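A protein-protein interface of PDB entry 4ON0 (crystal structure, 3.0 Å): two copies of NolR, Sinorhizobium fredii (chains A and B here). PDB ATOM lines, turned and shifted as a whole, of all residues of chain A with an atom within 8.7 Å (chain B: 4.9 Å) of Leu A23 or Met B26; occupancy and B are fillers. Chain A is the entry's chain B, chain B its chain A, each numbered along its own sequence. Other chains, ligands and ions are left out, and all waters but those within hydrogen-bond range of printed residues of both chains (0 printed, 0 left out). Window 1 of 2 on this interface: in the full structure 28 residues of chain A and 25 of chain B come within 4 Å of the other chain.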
ATOM      1  N   ALA A  16      14.350  34.039  24.465  1.00  0.00           N
ATOM      2  CA  ALA A  16      14.829  32.685  24.212  1.00  0.00           C
ATOM      3  C   ALA A  16      15.780  32.656  23.027  1.00  0.00           C
ATOM      4  O   ALA A  16      16.774  31.935  23.040  1.00  0.00           O
ATOM      5  CB  ALA A  16      13.663  31.745  23.967  1.00  0.00           C
ATOM      6  N   GLU A  17      15.474  33.452  22.008  1.00  0.00           N
ATOM      7  CA  GLU A  17      16.315  33.524  20.818  1.00  0.00           C
ATOM      8  C   GLU A  17      17.701  34.072  21.156  1.00  0.00           C
ATOM      9  O   GLU A  17      18.721  33.494  20.760  1.00  0.00           O
ATOM     10  CB  GLU A  17      15.644  34.378  19.741  1.00  0.00           C
ATOM     11  CG  GLU A  17      16.123  34.087  18.330  1.00  0.00           C
ATOM     12  CD  GLU A  17      15.167  34.612  17.273  1.00  0.00           C
ATOM     13  OE1 GLU A  17      14.202  35.319  17.635  1.00  0.00           O
ATOM     14  OE2 GLU A  17      15.381  34.311  16.081  1.00  0.00           O
ATOM     15  N   ILE A  18      17.734  35.177  21.900  1.00  0.00           N
ATOM     16  CA  ILE A  18      19.007  35.802  22.271  1.00  0.00           C
ATOM     17  C   ILE A  18      19.837  34.890  23.180  1.00  0.00           C
ATOM     18  O   ILE A  18      21.035  34.656  22.936  1.00  0.00           O
ATOM     19  CB  ILE A  18      18.783  37.149  22.983  1.00  0.00           C
ATOM     20  CG1 ILE A  18      18.063  38.129  22.053  1.00  0.00           C
ATOM     21  CG2 ILE A  18      20.107  37.723  23.469  1.00  0.00           C
ATOM     22  CD1 ILE A  18      17.269  39.199  22.774  1.00  0.00           C
ATOM     23  N   ALA A  19      19.186  34.378  24.221  1.00  0.00           N
ATOM     24  CA  ALA A  19      19.818  33.463  25.162  1.00  0.00           C
ATOM     25  C   ALA A  19      20.385  32.260  24.426  1.00  0.00           C
ATOM     26  O   ALA A  19      21.480  31.790  24.732  1.00  0.00           O
ATOM     27  CB  ALA A  19      18.825  33.019  26.221  1.00  0.00           C
ATOM     28  N   ALA A  20      19.630  31.766  23.450  1.00  0.00           N
ATOM     29  CA  ALA A  20      20.060  30.628  22.652  1.00  0.00           C
ATOM     30  C   ALA A  20      21.252  30.981  21.775  1.00  0.00           C
ATOM     31  O   ALA A  20      22.108  30.140  21.532  1.00  0.00           O
ATOM     32  CB  ALA A  20      18.919  30.114  21.801  1.00  0.00           C
ATOM     33  N   GLY A  21      21.305  32.217  21.290  1.00  0.00           N
ATOM     34  CA  GLY A  21      22.446  32.651  20.501  1.00  0.00           C
ATOM     35  C   GLY A  21      23.714  32.647  21.334  1.00  0.00           C
ATOM     36  O   GLY A  21      24.758  32.123  20.917  1.00  0.00           O
ATOM     37  N   PHE A  22      23.611  33.217  22.532  1.00  0.00           N
ATOM     38  CA  PHE A  22      24.718  33.231  23.485  1.00  0.00           C
ATOM     39  C   PHE A  22      25.186  31.817  23.852  1.00  0.00           C
ATOM     40  O   PHE A  22      26.375  31.470  23.725  1.00  0.00           O
ATOM     41  CB  PHE A  22      24.289  33.992  24.741  1.00  0.00           C
ATOM     42  CG  PHE A  22      25.170  33.758  25.931  1.00  0.00           C
ATOM     43  CD1 PHE A  22      26.526  34.034  25.881  1.00  0.00           C
ATOM     44  CD2 PHE A  22      24.636  33.262  27.106  1.00  0.00           C
ATOM     45  CE1 PHE A  22      27.329  33.816  26.981  1.00  0.00           C
ATOM     46  CE2 PHE A  22      25.433  33.041  28.207  1.00  0.00           C
ATOM     47  CZ  PHE A  22      26.782  33.317  28.145  1.00  0.00           C
ATOM     48  N   LEU A  23      24.234  31.001  24.291  1.00  0.00           N
ATOM     49  CA  LEU A  23      24.514  29.634  24.708  1.00  0.00           C
ATOM     50  C   LEU A  23      25.138  28.840  23.567  1.00  0.00           C
ATOM     51  O   LEU A  23      26.051  28.046  23.783  1.00  0.00           O
ATOM     52  CB  LEU A  23      23.228  28.953  25.182  1.00  0.00           C
ATOM     53  CG  LEU A  23      23.210  28.338  26.582  1.00  0.00           C
ATOM     54  CD1 LEU A  23      23.722  29.333  27.607  1.00  0.00           C
ATOM     55  CD2 LEU A  23      21.810  27.866  26.940  1.00  0.00           C
ATOM     56  N   SER A  24      24.654  29.080  22.351  1.00  0.00           N
ATOM     57  CA  SER A  24      25.195  28.433  21.162  1.00  0.00           C
ATOM     58  C   SER A  24      26.635  28.857  20.934  1.00  0.00           C
ATOM     59  O   SER A  24      27.463  28.057  20.503  1.00  0.00           O
ATOM     60  CB  SER A  24      24.354  28.758  19.928  1.00  0.00           C
ATOM     61  OG  SER A  24      22.975  28.542  20.172  1.00  0.00           O
ATOM     62  N   ALA A  25      26.930  30.123  21.217  1.00  0.00           N
ATOM     63  CA  ALA A  25      28.307  30.595  21.124  1.00  0.00           C
ATOM     64  C   ALA A  25      29.172  29.834  22.119  1.00  0.00           C
ATOM     65  O   ALA A  25      30.352  29.588  21.866  1.00  0.00           O
ATOM     66  CB  ALA A  25      28.394  32.087  21.376  1.00  0.00           C
ATOM     67  N   MET A  26      28.588  29.470  23.259  1.00  0.00           N
ATOM     68  CA  MET A  26      29.330  28.673  24.236  1.00  0.00           C
ATOM     69  C   MET A  26      29.194  27.151  24.055  1.00  0.00           C
ATOM     70  O   MET A  26      29.986  26.391  24.607  1.00  0.00           O
ATOM     71  CB  MET A  26      28.904  29.053  25.655  1.00  0.00           C
ATOM     72  CG  MET A  26      29.345  30.441  26.080  1.00  0.00           C
ATOM     73  SD  MET A  26      29.209  30.695  27.861  1.00  0.00           S
ATOM     74  CE  MET A  26      30.455  29.565  28.475  1.00  0.00           C
ATOM     75  N   ALA A  27      28.209  26.705  23.281  1.00  0.00           N
ATOM     76  CA  ALA A  27      27.914  25.270  23.182  1.00  0.00           C
ATOM     77  C   ALA A  27      28.853  24.509  22.240  1.00  0.00           C
ATOM     78  O   ALA A  27      28.405  23.873  21.285  1.00  0.00           O
ATOM     79  CB  ALA A  27      26.473  25.065  22.747  1.00  0.00           C
ATOM     80  N   ASN A  28      30.151  24.577  22.519  1.00  0.00           N
ATOM     81  CA  ASN A  28      31.159  23.831  21.766  1.00  0.00           C
ATOM     82  C   ASN A  28      32.348  23.520  22.678  1.00  0.00           C
ATOM     83  O   ASN A  28      32.738  24.360  23.488  1.00  0.00           O
ATOM     84  CB  ASN A  28      31.602  24.620  20.529  1.00  0.00           C
ATOM     85  CG  ASN A  28      32.731  23.941  19.772  1.00  0.00           C
ATOM     86  OD1 ASN A  28      33.905  24.068  20.130  1.00  0.00           O
ATOM     87  ND2 ASN A  28      32.381  23.221  18.711  1.00  0.00           N
ATOM     88  N   ARG A  31      35.575  25.662  22.027  1.00  0.00           N
ATOM     89  CA  ARG A  31      35.188  27.029  22.358  1.00  0.00           C
ATOM     90  C   ARG A  31      35.094  27.225  23.869  1.00  0.00           C
ATOM     91  O   ARG A  31      35.419  28.291  24.396  1.00  0.00           O
ATOM     92  CB  ARG A  31      33.852  27.367  21.703  1.00  0.00           C
ATOM     93  CG  ARG A  31      33.719  28.810  21.272  1.00  0.00           C
ATOM     94  CD  ARG A  31      33.157  28.900  19.868  1.00  0.00           C
ATOM     95  NE  ARG A  31      31.822  28.323  19.796  1.00  0.00           N
ATOM     96  CZ  ARG A  31      31.333  27.709  18.725  1.00  0.00           C
ATOM     97  NH1 ARG A  31      32.073  27.595  17.631  1.00  0.00           N
ATOM     98  NH2 ARG A  31      30.104  27.208  18.749  1.00  0.00           N
ATOM     99  N   LEU A  32      34.646  26.184  24.560  1.00  0.00           N
ATOM    100  CA  LEU A  32      34.541  26.203  26.013  1.00  0.00           C
ATOM    101  C   LEU A  32      35.923  26.267  26.652  1.00  0.00           C
ATOM    102  O   LEU A  32      36.155  27.042  27.588  1.00  0.00           O
ATOM    103  CB  LEU A  32      33.783  24.968  26.499  1.00  0.00           C
ATOM    104  CG  LEU A  32      32.655  25.185  27.507  1.00  0.00           C
ATOM    105  CD1 LEU A  32      31.867  26.437  27.166  1.00  0.00           C
ATOM    106  CD2 LEU A  32      31.742  23.968  27.529  1.00  0.00           C
ATOM    107  N   LEU A  35      37.215  29.795  26.142  1.00  0.00           N
ATOM    108  CA  LEU A  35      36.657  30.768  27.075  1.00  0.00           C
ATOM    109  C   LEU A  35      37.195  30.593  28.487  1.00  0.00           C
ATOM    110  O   LEU A  35      37.428  31.578  29.183  1.00  0.00           O
ATOM    111  CB  LEU A  35      35.131  30.686  27.087  1.00  0.00           C
ATOM    112  CG  LEU A  35      34.452  31.252  25.840  1.00  0.00           C
ATOM    113  CD1 LEU A  35      32.957  31.044  25.925  1.00  0.00           C
ATOM    114  CD2 LEU A  35      34.787  32.728  25.695  1.00  0.00           C
ATOM    115  N   LEU A  66      33.147  33.903  18.709  1.00  0.00           N
ATOM    116  CA  LEU A  66      33.066  34.442  20.065  1.00  0.00           C
ATOM    117  C   LEU A  66      32.942  35.965  20.030  1.00  0.00           C
ATOM    118  O   LEU A  66      32.193  36.551  20.810  1.00  0.00           O
ATOM    119  CB  LEU A  66      34.279  34.029  20.895  1.00  0.00           C
ATOM    120  CG  LEU A  66      34.316  32.585  21.392  1.00  0.00           C
ATOM    121  CD1 LEU A  66      35.622  32.311  22.121  1.00  0.00           C
ATOM    122  CD2 LEU A  66      33.134  32.319  22.306  1.00  0.00           C
ATOM    123  N   GLN A  69      29.422  37.282  19.320  1.00  0.00           N
ATOM    124  CA  GLN A  69      28.515  37.355  20.457  1.00  0.00           C
ATOM    125  C   GLN A  69      29.049  38.272  21.557  1.00  0.00           C
ATOM    126  O   GLN A  69      28.487  38.323  22.655  1.00  0.00           O
ATOM    127  CB  GLN A  69      28.251  35.954  21.002  1.00  0.00           C
ATOM    128  CG  GLN A  69      27.264  35.176  20.162  1.00  0.00           C
ATOM    129  CD  GLN A  69      25.843  35.659  20.337  1.00  0.00           C
ATOM    130  OE1 GLN A  69      25.404  35.948  21.449  1.00  0.00           O
ATOM    131  NE2 GLN A  69      25.112  35.751  19.233  1.00  0.00           N
ATOM    132  N   LEU A  71      31.872  38.051  23.269  1.00  0.00           N
ATOM    133  CA  LEU A  71      32.269  37.224  24.393  1.00  0.00           C
ATOM    134  C   LEU A  71      33.763  37.343  24.713  1.00  0.00           C
ATOM    135  O   LEU A  71      34.227  36.797  25.713  1.00  0.00           O
ATOM    136  CB  LEU A  71      31.908  35.768  24.096  1.00  0.00           C
ATOM    137  CG  LEU A  71      30.463  35.348  24.391  1.00  0.00           C
ATOM    138  CD1 LEU A  71      30.349  33.838  24.522  1.00  0.00           C
ATOM    139  CD2 LEU A  71      29.895  36.051  25.611  1.00  0.00           C
ATOM    140  N   SER A  89      28.678  37.150  31.587  1.00  0.00           N
ATOM    141  CA  SER A  89      27.849  36.035  31.151  1.00  0.00           C
ATOM    142  C   SER A  89      28.657  34.741  31.082  1.00  0.00           C
ATOM    143  O   SER A  89      28.226  33.694  31.584  1.00  0.00           O
ATOM    144  CB  SER A  89      27.224  36.344  29.792  1.00  0.00           C
ATOM    145  OG  SER A  89      26.492  37.556  29.837  1.00  0.00           O
ATOM    146  N   VAL A  90      29.829  34.821  30.459  1.00  0.00           N
ATOM    147  CA  VAL A  90      30.713  33.667  30.342  1.00  0.00           C
ATOM    148  C   VAL A  90      31.099  33.144  31.717  1.00  0.00           C
ATOM    149  O   VAL A  90      31.049  31.944  31.958  1.00  0.00           O
ATOM    150  CB  VAL A  90      31.992  33.995  29.546  1.00  0.00           C
ATOM    151  CG1 VAL A  90      32.960  32.822  29.582  1.00  0.00           C
ATOM    152  CG2 VAL A  90      31.649  34.353  28.116  1.00  0.00           C
ATOM    153  N   LYS A  92      29.519  33.513  34.519  1.00  0.00           N
ATOM    154  CA  LYS A  92      28.335  32.963  35.169  1.00  0.00           C
ATOM    155  C   LYS A  92      28.061  31.543  34.688  1.00  0.00           C
ATOM    156  O   LYS A  92      27.837  30.635  35.492  1.00  0.00           O
ATOM    157  CB  LYS A  92      27.121  33.855  34.914  1.00  0.00           C
ATOM    158  CG  LYS A  92      27.075  35.096  35.791  1.00  0.00           C
ATOM    159  CD  LYS A  92      25.752  35.831  35.646  1.00  0.00           C
ATOM    160  CE  LYS A  92      25.829  37.226  36.245  1.00  0.00           C
ATOM    161  NZ  LYS A  92      24.658  38.066  35.865  1.00  0.00           N
ATOM    162  N   ILE A  93      28.073  31.363  33.370  1.00  0.00           N
ATOM    163  CA  ILE A  93      27.836  30.052  32.776  1.00  0.00           C
ATOM    164  C   ILE A  93      28.911  29.046  33.184  1.00  0.00           C
ATOM    165  O   ILE A  93      28.606  27.913  33.553  1.00  0.00           O
ATOM    166  CB  ILE A  93      27.777  30.136  31.243  1.00  0.00           C
ATOM    167  CG1 ILE A  93      26.585  30.986  30.816  1.00  0.00           C
ATOM    168  CG2 ILE A  93      27.660  28.750  30.638  1.00  0.00           C
ATOM    169  CD1 ILE A  93      25.250  30.368  31.169  1.00  0.00           C
ATOM    170  N   LEU A  94      30.170  29.467  33.108  1.00  0.00           N
ATOM    171  CA  LEU A  94      31.290  28.627  33.513  1.00  0.00           C
ATOM    172  C   LEU A  94      31.191  28.280  34.998  1.00  0.00           C
ATOM    173  O   LEU A  94      31.524  27.166  35.408  1.00  0.00           O
ATOM    174  CB  LEU A  94      32.624  29.324  33.217  1.00  0.00           C
ATOM    175  CG  LEU A  94      33.016  29.511  31.745  1.00  0.00           C
ATOM    176  CD1 LEU A  94      34.403  30.125  31.626  1.00  0.00           C
ATOM    177  CD2 LEU A  94      32.933  28.209  30.962  1.00  0.00           C
ATOM    178  N   LEU A  97      28.545  25.659  35.373  1.00  0.00           N
ATOM    179  CA  LEU A  97      29.124  24.420  34.866  1.00  0.00           C
ATOM    180  C   LEU A  97      30.066  23.780  35.886  1.00  0.00           C
ATOM    181  O   LEU A  97      30.093  22.558  36.040  1.00  0.00           O
ATOM    182  CB  LEU A  97      29.864  24.684  33.553  1.00  0.00           C
ATOM    183  CG  LEU A  97      28.991  24.731  32.297  1.00  0.00           C
ATOM    184  CD1 LEU A  97      29.840  24.958  31.054  1.00  0.00           C
ATOM    185  CD2 LEU A  97      28.178  23.455  32.162  1.00  0.00           C
ATOM    186  N   ILE A 100      28.049  22.226  38.537  1.00  0.00           N
ATOM    187  CA  ILE A 100      27.455  20.972  38.085  1.00  0.00           C
ATOM    188  C   ILE A 100      28.447  19.813  38.119  1.00  0.00           C
ATOM    189  O   ILE A 100      28.287  18.874  38.899  1.00  0.00           O
ATOM    190  CB  ILE A 100      26.888  21.112  36.663  1.00  0.00           C
ATOM    191  CG1 ILE A 100      25.774  22.160  36.638  1.00  0.00           C
ATOM    192  CG2 ILE A 100      26.364  19.775  36.164  1.00  0.00           C
ATOM    193  CD1 ILE A 100      25.346  22.563  35.246  1.00  0.00           C
ATOM    194  N   PHE B  22      25.894  18.969  26.832  1.00  0.00           N
ATOM    195  CA  PHE B  22      24.808  19.471  27.665  1.00  0.00           C
ATOM    196  C   PHE B  22      24.322  20.844  27.178  1.00  0.00           C
ATOM    197  O   PHE B  22      23.122  21.048  26.915  1.00  0.00           O
ATOM    198  CB  PHE B  22      25.275  19.532  29.121  1.00  0.00           C
ATOM    199  CG  PHE B  22      24.389  20.341  30.017  1.00  0.00           C
ATOM    200  CD1 PHE B  22      23.046  20.036  30.148  1.00  0.00           C
ATOM    201  CD2 PHE B  22      24.908  21.393  30.751  1.00  0.00           C
ATOM    202  CE1 PHE B  22      22.234  20.777  30.981  1.00  0.00           C
ATOM    203  CE2 PHE B  22      24.103  22.134  31.586  1.00  0.00           C
ATOM    204  CZ  PHE B  22      22.761  21.825  31.702  1.00  0.00           C
ATOM    205  N   LEU B  23      25.258  21.779  27.043  1.00  0.00           N
ATOM    206  CA  LEU B  23      24.921  23.124  26.588  1.00  0.00           C
ATOM    207  C   LEU B  23      24.271  23.101  25.208  1.00  0.00           C
ATOM    208  O   LEU B  23      23.359  23.879  24.941  1.00  0.00           O
ATOM    209  CB  LEU B  23      26.161  24.014  26.568  1.00  0.00           C
ATOM    210  CG  LEU B  23      26.648  24.471  27.943  1.00  0.00           C
ATOM    211  CD1 LEU B  23      27.901  25.316  27.815  1.00  0.00           C
ATOM    212  CD2 LEU B  23      25.555  25.243  28.661  1.00  0.00           C
ATOM    213  N   SER B  24      24.737  22.206  24.342  1.00  0.00           N
ATOM    214  CA  SER B  24      24.156  22.049  23.012  1.00  0.00           C
ATOM    215  C   SER B  24      22.718  21.575  23.131  1.00  0.00           C
ATOM    216  O   SER B  24      21.860  21.971  22.341  1.00  0.00           O
ATOM    217  CB  SER B  24      24.966  21.066  22.159  1.00  0.00           C
ATOM    218  OG  SER B  24      26.348  21.373  22.173  1.00  0.00           O
ATOM    219  N   ALA B  25      22.457  20.718  24.113  1.00  0.00           N
ATOM    220  CA  ALA B  25      21.087  20.286  24.376  1.00  0.00           C
ATOM    221  C   ALA B  25      20.233  21.476  24.800  1.00  0.00           C
ATOM    222  O   ALA B  25      19.041  21.540  24.485  1.00  0.00           O
ATOM    223  CB  ALA B  25      21.053  19.201  25.440  1.00  0.00           C
ATOM    224  N   MET B  26      20.839  22.422  25.511  1.00  0.00           N
ATOM    225  CA  MET B  26      20.099  23.619  25.909  1.00  0.00           C
ATOM    226  C   MET B  26      20.173  24.790  24.913  1.00  0.00           C
ATOM    227  O   MET B  26      19.378  25.725  25.002  1.00  0.00           O
ATOM    228  CB  MET B  26      20.577  24.093  27.283  1.00  0.00           C
ATOM    229  CG  MET B  26      20.202  23.156  28.421  1.00  0.00           C
ATOM    230  SD  MET B  26      20.386  23.934  30.036  1.00  0.00           S
ATOM    231  CE  MET B  26      19.091  25.169  29.950  1.00  0.00           C
ATOM    232  N   ALA B  27      21.111  24.742  23.969  1.00  0.00           N
ATOM    233  CA  ALA B  27      21.363  25.885  23.079  1.00  0.00           C
ATOM    234  C   ALA B  27      20.369  26.013  21.922  1.00  0.00           C
ATOM    235  O   ALA B  27      20.762  26.042  20.753  1.00  0.00           O
ATOM    236  CB  ALA B  27      22.784  25.811  22.528  1.00  0.00           C
ATOM    237  N   ASN B  28      19.087  26.112  22.254  1.00  0.00           N
ATOM    238  CA  ASN B  28      18.037  26.322  21.264  1.00  0.00           C
ATOM    239  C   ASN B  28      16.881  27.098  21.885  1.00  0.00           C
ATOM    240  O   ASN B  28      16.505  26.835  23.027  1.00  0.00           O
ATOM    241  CB  ASN B  28      17.558  24.977  20.706  1.00  0.00           C
ATOM    242  CG  ASN B  28      16.366  25.114  19.778  1.00  0.00           C
ATOM    243  OD1 ASN B  28      15.223  25.192  20.227  1.00  0.00           O
ATOM    244  ND2 ASN B  28      16.627  25.149  18.477  1.00  0.00           N
ATOM    245  N   LEU B  32      14.700  25.990  24.934  1.00  0.00           N
ATOM    246  CA  LEU B  32      14.844  26.780  26.151  1.00  0.00           C
ATOM    247  C   LEU B  32      13.483  27.098  26.770  1.00  0.00           C
ATOM    248  O   LEU B  32      13.297  26.958  27.984  1.00  0.00           O
ATOM    249  CB  LEU B  32      15.610  28.069  25.851  1.00  0.00           C
ATOM    250  CG  LEU B  32      16.765  28.415  26.785  1.00  0.00           C
ATOM    251  CD1 LEU B  32      17.538  27.165  27.167  1.00  0.00           C
ATOM    252  CD2 LEU B  32      17.680  29.424  26.113  1.00  0.00           C
ATOM    253  N   LEU B  35      12.216  23.833  28.281  1.00  0.00           N
ATOM    254  CA  LEU B  35      12.848  23.498  29.553  1.00  0.00           C
ATOM    255  C   LEU B  35      12.384  24.407  30.680  1.00  0.00           C
ATOM    256  O   LEU B  35      12.213  23.950  31.803  1.00  0.00           O
ATOM    257  CB  LEU B  35      14.369  23.562  29.439  1.00  0.00           C
ATOM    258  CG  LEU B  35      15.035  22.432  28.660  1.00  0.00           C
ATOM    259  CD1 LEU B  35      16.527  22.676  28.570  1.00  0.00           C
ATOM    260  CD2 LEU B  35      14.749  21.103  29.330  1.00  0.00           C
ATOM    261  N   LEU B  71      17.473  15.187  30.345  1.00  0.00           N
ATOM    262  CA  LEU B  71      17.117  16.475  30.936  1.00  0.00           C
ATOM    263  C   LEU B  71      15.625  16.553  31.264  1.00  0.00           C
ATOM    264  O   LEU B  71      15.166  17.540  31.843  1.00  0.00           O
ATOM    265  CB  LEU B  71      17.497  17.629  30.005  1.00  0.00           C
ATOM    266  CG  LEU B  71      18.886  18.269  30.090  1.00  0.00           C
ATOM    267  CD1 LEU B  71      19.999  17.245  30.172  1.00  0.00           C
ATOM    268  CD2 LEU B  71      19.098  19.184  28.895  1.00  0.00           C
ATOM    269  N   VAL B  90      19.914  21.931  34.694  1.00  0.00           N
ATOM    270  CA  VAL B  90      19.031  22.767  33.891  1.00  0.00           C
ATOM    271  C   VAL B  90      18.634  24.015  34.670  1.00  0.00           C
ATOM    272  O   VAL B  90      18.669  25.125  34.144  1.00  0.00           O
ATOM    273  CB  VAL B  90      17.761  22.007  33.470  1.00  0.00           C
ATOM    274  CG1 VAL B  90      16.781  22.943  32.781  1.00  0.00           C
ATOM    275  CG2 VAL B  90      18.118  20.832  32.573  1.00  0.00           C
ATOM    276  N   ILE B  93      21.628  26.454  34.910  1.00  0.00           N
ATOM    277  CA  ILE B  93      21.847  27.197  33.672  1.00  0.00           C
ATOM    278  C   ILE B  93      20.761  28.250  33.460  1.00  0.00           C
ATOM    279  O   ILE B  93      21.061  29.404  33.151  1.00  0.00           O
ATOM    280  CB  ILE B  93      21.890  26.259  32.447  1.00  0.00           C
ATOM    281  CG1 ILE B  93      23.077  25.303  32.548  1.00  0.00           C
ATOM    282  CG2 ILE B  93      21.981  27.064  31.160  1.00  0.00           C
ATOM    283  CD1 ILE B  93      24.423  25.986  32.469  1.00  0.00           C
ATOM    284  N   LEU B  94      19.504  27.852  33.639  1.00  0.00           N
ATOM    285  CA  LEU B  94      18.381  28.777  33.516  1.00  0.00           C
ATOM    286  C   LEU B  94      18.479  29.892  34.549  1.00  0.00           C
ATOM    287  O   LEU B  94      18.124  31.037  34.270  1.00  0.00           O
ATOM    288  CB  LEU B  94      17.046  28.041  33.667  1.00  0.00           C
ATOM    289  CG  LEU B  94      16.631  27.097  32.538  1.00  0.00           C
ATOM    290  CD1 LEU B  94      15.249  26.519  32.803  1.00  0.00           C
ATOM    291  CD2 LEU B  94      16.657  27.822  31.205  1.00  0.00           C
ATOM    292  N   LEU B  97      21.041  32.294  33.294  1.00  0.00           N
ATOM    293  CA  LEU B  97      20.450  33.006  32.165  1.00  0.00           C
ATOM    294  C   LEU B  97      19.490  34.100  32.622  1.00  0.00           C
ATOM    295  O   LEU B  97      19.458  35.190  32.049  1.00  0.00           O
ATOM    296  CB  LEU B  97      19.722  32.020  31.251  1.00  0.00           C
ATOM    297  CG  LEU B  97      20.570  31.249  30.240  1.00  0.00           C
ATOM    298  CD1 LEU B  97      19.693  30.343  29.389  1.00  0.00           C
ATOM    299  CD2 LEU B  97      21.352  32.210  29.363  1.00  0.00           C
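The backbone carbonyl oxygen of Ala A27 is in hydrogen-bond range of the side-chain hydroxyl of Ser B24 (3.4 Å).
The side-chain hydroxyl of Ser A24 lies within hydrogen-bond range of the backbone carbonyl oxygen of Ala B27 (3.4 Å).
Leu A23 touches Met B26, and with the chains exchanged Met A26 touches Leu B23.
Leu A23 touches Ala B27, and with the chains exchanged Ala A27 touches Leu B23.
Ser A24 touches Ala B27, and with the chains exchanged Ala A27 touches Ser B24.
Ala A27 touches its own counterpart, Ala B27.
Hydrophobic or aromatic side chains of chain A within 4 Å of the printed part of chain B: Ala A19, Ala A20, Leu A23, Ala A27, Leu A97 and Ile A100.
Along chain A the printed residues that touch a printed residue of chain B span positions 19 to 100.
Among the printed residues, 11 pairs touch across the chains.
CD2 of Leu B32 touches CB of Ala A19 (3.8 Å).
Asn B28 touches Ala A20 (C to CB, 3.6 Å).
Leu A23 touches Met B26.
C of Leu A23 touches CB of Ala B27 (3.97 Å).
Met A26 touches Leu B23 (O to CD1, 3.97 Å).
C of Leu B23 touches CB of Ala A27, 3.8 Å away.
CB of Ala A27 touches CB of Ala B27 (3.8 Å).
Leu B23 touches Leu A97 (CD1 to CD1, 3.8 Å).
Ile A100 touches Phe B22 (CD1 to CE2, 3.9 Å).
Leu A23 touches just these residues of chain B: Met B26 and Ala B27.
Of the printed residues of chain B, Ala A27 touches Leu B23, Ser B24 and Ala B27.
Printed residues of chain B within 4 Å of Ile A100: Phe B22 (3.9 Å).
Of the printed residues of chain A, Leu B23 touches Met A26, Ala A27 and Leu A97.
No residue of chain A comes within 4 Å of Ala B25.
Of the printed residues of chain A, Leu B32 touches Ala A19.
Leu B94 touches none of the printed residues of chain A.
The nearest printed residue of chain A that does not touch Leu B23 is Leu A32 (4.1 Å).
O of Ser A24 lies within hydrogen-bond range of NH2 of Arg A31, 3.3 Å away.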
